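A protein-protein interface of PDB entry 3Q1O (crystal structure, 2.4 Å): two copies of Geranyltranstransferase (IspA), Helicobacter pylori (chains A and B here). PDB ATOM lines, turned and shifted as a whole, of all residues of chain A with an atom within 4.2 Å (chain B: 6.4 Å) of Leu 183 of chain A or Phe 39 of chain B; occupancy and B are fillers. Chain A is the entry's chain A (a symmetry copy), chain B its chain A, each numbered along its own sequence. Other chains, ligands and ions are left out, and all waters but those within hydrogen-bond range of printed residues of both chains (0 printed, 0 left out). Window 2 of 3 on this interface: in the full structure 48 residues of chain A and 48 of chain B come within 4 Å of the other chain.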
ATOM      1  N   LEU A 174      25.788 -27.442  15.778  1.00  0.00           N
ATOM      2  CA  LEU A 174      25.458 -27.515  17.205  1.00  0.00           C
ATOM      3  C   LEU A 174      26.721 -27.540  18.043  1.00  0.00           C
ATOM      4  O   LEU A 174      26.861 -26.759  18.987  1.00  0.00           O
ATOM      5  CB  LEU A 174      24.595 -28.739  17.526  1.00  0.00           C
ATOM      6  CG  LEU A 174      23.122 -28.679  17.118  1.00  0.00           C
ATOM      7  CD1 LEU A 174      22.464 -30.032  17.317  1.00  0.00           C
ATOM      8  CD2 LEU A 174      22.361 -27.587  17.858  1.00  0.00           C
ATOM      9  N   PHE A 178      27.414 -24.262  20.513  1.00  0.00           N
ATOM     10  CA  PHE A 178      27.324 -24.490  21.949  1.00  0.00           C
ATOM     11  C   PHE A 178      28.643 -24.934  22.552  1.00  0.00           C
ATOM     12  O   PHE A 178      28.641 -25.614  23.569  1.00  0.00           O
ATOM     13  CB  PHE A 178      26.230 -25.514  22.260  1.00  0.00           C
ATOM     14  CG  PHE A 178      24.854 -25.022  21.960  1.00  0.00           C
ATOM     15  CD1 PHE A 178      24.225 -24.114  22.806  1.00  0.00           C
ATOM     16  CD2 PHE A 178      24.181 -25.452  20.825  1.00  0.00           C
ATOM     17  CE1 PHE A 178      22.942 -23.645  22.528  1.00  0.00           C
ATOM     18  CE2 PHE A 178      22.901 -24.987  20.531  1.00  0.00           C
ATOM     19  CZ  PHE A 178      22.276 -24.084  21.388  1.00  0.00           C
ATOM     20  N   THR A 181      28.561 -23.287  26.031  1.00  0.00           N
ATOM     21  CA  THR A 181      27.390 -23.718  26.793  1.00  0.00           C
ATOM     22  C   THR A 181      27.516 -25.197  27.184  1.00  0.00           C
ATOM     23  O   THR A 181      27.761 -26.042  26.326  1.00  0.00           O
ATOM     24  CB  THR A 181      26.092 -23.514  25.981  1.00  0.00           C
ATOM     25  OG1 THR A 181      26.105 -22.224  25.361  1.00  0.00           O
ATOM     26  CG2 THR A 181      24.860 -23.628  26.876  1.00  0.00           C
ATOM     27  N   PRO A 182      27.375 -25.515  28.488  1.00  0.00           N
ATOM     28  CA  PRO A 182      27.348 -26.930  28.856  1.00  0.00           C
ATOM     29  C   PRO A 182      25.957 -27.498  28.602  1.00  0.00           C
ATOM     30  O   PRO A 182      24.958 -26.956  29.085  1.00  0.00           O
ATOM     31  CB  PRO A 182      27.676 -26.924  30.358  1.00  0.00           C
ATOM     32  CG  PRO A 182      28.057 -25.505  30.692  1.00  0.00           C
ATOM     33  CD  PRO A 182      27.372 -24.649  29.677  1.00  0.00           C
ATOM     34  N   LEU A 183      25.901 -28.572  27.825  1.00  0.00           N
ATOM     35  CA  LEU A 183      24.631 -29.166  27.423  1.00  0.00           C
ATOM     36  C   LEU A 183      24.263 -30.302  28.360  1.00  0.00           C
ATOM     37  O   LEU A 183      25.127 -30.853  29.044  1.00  0.00           O
ATOM     38  CB  LEU A 183      24.732 -29.690  25.989  1.00  0.00           C
ATOM     39  CG  LEU A 183      25.034 -28.681  24.882  1.00  0.00           C
ATOM     40  CD1 LEU A 183      25.408 -29.406  23.591  1.00  0.00           C
ATOM     41  CD2 LEU A 183      23.848 -27.740  24.672  1.00  0.00           C
ATOM     42  N   ASN A 184      22.982 -30.660  28.394  1.00  0.00           N
ATOM     43  CA  ASN A 184      22.594 -31.863  29.121  1.00  0.00           C
ATOM     44  C   ASN A 184      22.869 -33.130  28.293  1.00  0.00           C
ATOM     45  O   ASN A 184      23.303 -33.037  27.136  1.00  0.00           O
ATOM     46  CB  ASN A 184      21.151 -31.779  29.654  1.00  0.00           C
ATOM     47  CG  ASN A 184      20.102 -31.728  28.564  1.00  0.00           C
ATOM     48  OD1 ASN A 184      20.118 -32.507  27.607  1.00  0.00           O
ATOM     49  ND2 ASN A 184      19.152 -30.823  28.727  1.00  0.00           N
ATOM     50  N   GLN A 187      20.786 -33.534  25.054  1.00  0.00           N
ATOM     51  CA  GLN A 187      21.226 -32.611  24.006  1.00  0.00           C
ATOM     52  C   GLN A 187      22.528 -33.070  23.347  1.00  0.00           C
ATOM     53  O   GLN A 187      22.653 -33.034  22.128  1.00  0.00           O
ATOM     54  CB  GLN A 187      21.376 -31.204  24.570  1.00  0.00           C
ATOM     55  CG  GLN A 187      20.042 -30.534  24.871  1.00  0.00           C
ATOM     56  CD  GLN A 187      20.189 -29.298  25.740  1.00  0.00           C
ATOM     57  OE1 GLN A 187      21.090 -29.213  26.581  1.00  0.00           O
ATOM     58  NE2 GLN A 187      19.308 -28.331  25.537  1.00  0.00           N
ATOM     59  N   PHE A 190      21.799 -36.014  21.133  1.00  0.00           N
ATOM     60  CA  PHE A 190      21.206 -35.508  19.891  1.00  0.00           C
ATOM     61  C   PHE A 190      22.291 -35.009  18.938  1.00  0.00           C
ATOM     62  O   PHE A 190      22.290 -35.340  17.745  1.00  0.00           O
ATOM     63  CB  PHE A 190      20.223 -34.381  20.219  1.00  0.00           C
ATOM     64  CG  PHE A 190      19.496 -33.814  19.021  1.00  0.00           C
ATOM     65  CD1 PHE A 190      20.037 -32.742  18.290  1.00  0.00           C
ATOM     66  CD2 PHE A 190      18.249 -34.313  18.652  1.00  0.00           C
ATOM     67  CE1 PHE A 190      19.357 -32.201  17.193  1.00  0.00           C
ATOM     68  CE2 PHE A 190      17.556 -33.771  17.560  1.00  0.00           C
ATOM     69  CZ  PHE A 190      18.109 -32.715  16.829  1.00  0.00           C
ATOM     70  N   LEU A 191      23.211 -34.220  19.484  1.00  0.00           N
ATOM     71  CA  LEU A 191      24.321 -33.657  18.742  1.00  0.00           C
ATOM     72  C   LEU A 191      25.165 -34.770  18.111  1.00  0.00           C
ATOM     73  O   LEU A 191      25.398 -34.758  16.905  1.00  0.00           O
ATOM     74  CB  LEU A 191      25.157 -32.782  19.684  1.00  0.00           C
ATOM     75  CG  LEU A 191      26.309 -31.908  19.189  1.00  0.00           C
ATOM     76  CD1 LEU A 191      26.478 -30.731  20.147  1.00  0.00           C
ATOM     77  CD2 LEU A 191      27.612 -32.687  19.101  1.00  0.00           C
ATOM     78  N   ASN A 260      32.166 -29.784  24.043  1.00  0.00           N
ATOM     79  CA  ASN A 260      31.143 -30.708  24.538  1.00  0.00           C
ATOM     80  C   ASN A 260      31.369 -32.170  24.169  1.00  0.00           C
ATOM     81  O   ASN A 260      31.157 -32.575  23.024  1.00  0.00           O
ATOM     82  CB  ASN A 260      29.754 -30.265  24.082  1.00  0.00           C
ATOM     83  CG  ASN A 260      29.014 -29.487  25.147  1.00  0.00           C
ATOM     84  OD1 ASN A 260      28.857 -29.950  26.277  1.00  0.00           O
ATOM     85  ND2 ASN A 260      28.543 -28.302  24.789  1.00  0.00           N
ATOM     86  N   LEU A 265      31.161 -34.172  30.218  1.00  0.00           N
ATOM     87  CA  LEU A 265      29.850 -34.169  30.838  1.00  0.00           C
ATOM     88  C   LEU A 265      29.747 -35.124  32.021  1.00  0.00           C
ATOM     89  O   LEU A 265      29.241 -34.750  33.072  1.00  0.00           O
ATOM     90  CB  LEU A 265      28.787 -34.513  29.803  1.00  0.00           C
ATOM     91  CG  LEU A 265      27.412 -33.984  30.200  1.00  0.00           C
ATOM     92  CD1 LEU A 265      27.456 -32.454  30.272  1.00  0.00           C
ATOM     93  CD2 LEU A 265      26.363 -34.460  29.225  1.00  0.00           C
ATOM     94  N   GLU B  37      14.246 -29.369  12.823  1.00  0.00           N
ATOM     95  CA  GLU B  37      13.928 -29.431  14.237  1.00  0.00           C
ATOM     96  C   GLU B  37      15.223 -29.657  14.990  1.00  0.00           C
ATOM     97  O   GLU B  37      15.850 -30.713  14.849  1.00  0.00           O
ATOM     98  CB  GLU B  37      12.955 -30.572  14.543  1.00  0.00           C
ATOM     99  CG  GLU B  37      11.845 -30.771  13.523  1.00  0.00           C
ATOM    100  CD  GLU B  37      11.251 -32.164  13.599  1.00  0.00           C
ATOM    101  OE1 GLU B  37      10.582 -32.475  14.611  1.00  0.00           O
ATOM    102  OE2 GLU B  37      11.457 -32.950  12.646  1.00  0.00           O
ATOM    103  N   SER B  38      15.623 -28.652  15.767  1.00  0.00           N
ATOM    104  CA  SER B  38      16.788 -28.743  16.643  1.00  0.00           C
ATOM    105  C   SER B  38      16.770 -27.613  17.654  1.00  0.00           C
ATOM    106  O   SER B  38      15.954 -26.699  17.557  1.00  0.00           O
ATOM    107  CB  SER B  38      18.088 -28.641  15.841  1.00  0.00           C
ATOM    108  OG  SER B  38      18.422 -27.283  15.571  1.00  0.00           O
ATOM    109  N   PHE B  39      17.712 -27.652  18.588  1.00  0.00           N
ATOM    110  CA  PHE B  39      17.864 -26.581  19.563  1.00  0.00           C
ATOM    111  C   PHE B  39      18.896 -25.520  19.139  1.00  0.00           C
ATOM    112  O   PHE B  39      19.394 -24.761  19.979  1.00  0.00           O
ATOM    113  CB  PHE B  39      18.138 -27.147  20.977  1.00  0.00           C
ATOM    114  CG  PHE B  39      19.359 -28.014  21.068  1.00  0.00           C
ATOM    115  CD1 PHE B  39      20.571 -27.482  21.486  1.00  0.00           C
ATOM    116  CD2 PHE B  39      19.298 -29.370  20.753  1.00  0.00           C
ATOM    117  CE1 PHE B  39      21.709 -28.274  21.570  1.00  0.00           C
ATOM    118  CE2 PHE B  39      20.427 -30.167  20.834  1.00  0.00           C
ATOM    119  CZ  PHE B  39      21.637 -29.616  21.244  1.00  0.00           C
ATOM    120  N   HIS B  40      19.207 -25.466  17.841  1.00  0.00           N
ATOM    121  CA  HIS B  40      19.997 -24.361  17.278  1.00  0.00           C
ATOM    122  C   HIS B  40      19.078 -23.161  17.030  1.00  0.00           C
ATOM    123  O   HIS B  40      18.040 -23.306  16.384  1.00  0.00           O
ATOM    124  CB  HIS B  40      20.685 -24.775  15.974  1.00  0.00           C
ATOM    125  CG  HIS B  40      21.853 -23.911  15.605  1.00  0.00           C
ATOM    126  ND1 HIS B  40      21.710 -22.626  15.122  1.00  0.00           N
ATOM    127  CD2 HIS B  40      23.187 -24.149  15.648  1.00  0.00           C
ATOM    128  CE1 HIS B  40      22.905 -22.110  14.886  1.00  0.00           C
ATOM    129  NE2 HIS B  40      23.817 -23.012  15.200  1.00  0.00           N
ATOM    130  N   PRO B  41      19.457 -21.972  17.538  1.00  0.00           N
ATOM    131  CA  PRO B  41      18.586 -20.790  17.455  1.00  0.00           C
ATOM    132  C   PRO B  41      18.328 -20.263  16.039  1.00  0.00           C
ATOM    133  O   PRO B  41      17.247 -19.725  15.785  1.00  0.00           O
ATOM    134  CB  PRO B  41      19.341 -19.726  18.268  1.00  0.00           C
ATOM    135  CG  PRO B  41      20.354 -20.463  19.050  1.00  0.00           C
ATOM    136  CD  PRO B  41      20.711 -21.674  18.253  1.00  0.00           C
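The side-chain amide oxygen of Asn 184 of chain A lies within hydrogen-bond range of the backbone NH of Gln 187 of chain A (2.8 Å). OG of Ser 38 of chain B is in hydrogen-bond range of N of His 40 of chain B, 3.0 Å away. O of Phe 178 of chain A sits at hydrogen-bond distance from ND2 of Asn 260 of chain A (3.0 Å).
Among the printed residues, 7 pairs touch across the chains.
No position is printed for both chains.
Among the printed residues, pairs that only touch across the chains: Phe 178 of chain A with Phe 39 of chain B (3.3 Å), Phe 190 of chain A with Glu 37 of chain B (3.6 Å), Phe 190 of chain A with Phe 39 of chain B (3.6 Å), Gln 187 of chain A with Phe 39 of chain B (3.7 Å), Leu 174 of chain A with His 40 of chain B (3.8 Å), Leu 183 of chain A with Phe 39 of chain B (3.8 Å) and Leu 174 of chain A with Phe 39 of chain B (3.8 Å).
Printed residues of chain B within 4 Å of Leu 174 of chain A: Phe 39 (3.8 Å) and His 40 (3.8 Å). Of the printed residues of chain B, Phe 178 of chain A touches Phe 39 (3.3 Å). Of the printed residues of chain B, Phe 190 of chain A touches Glu 37 (3.6 Å) and Phe 39 (3.6 Å). Of the printed residues of chain A, Glu 37 of chain B touches Phe 190. Phe 39 of chain B touches five residues of chain A. Of the printed residues of chain A, His 40 of chain B touches Leu 174 (3.8 Å). The nearest printed residue of chain B that does not touch Phe 190 of chain A is Ser 38 of chain B (4.01 Å).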
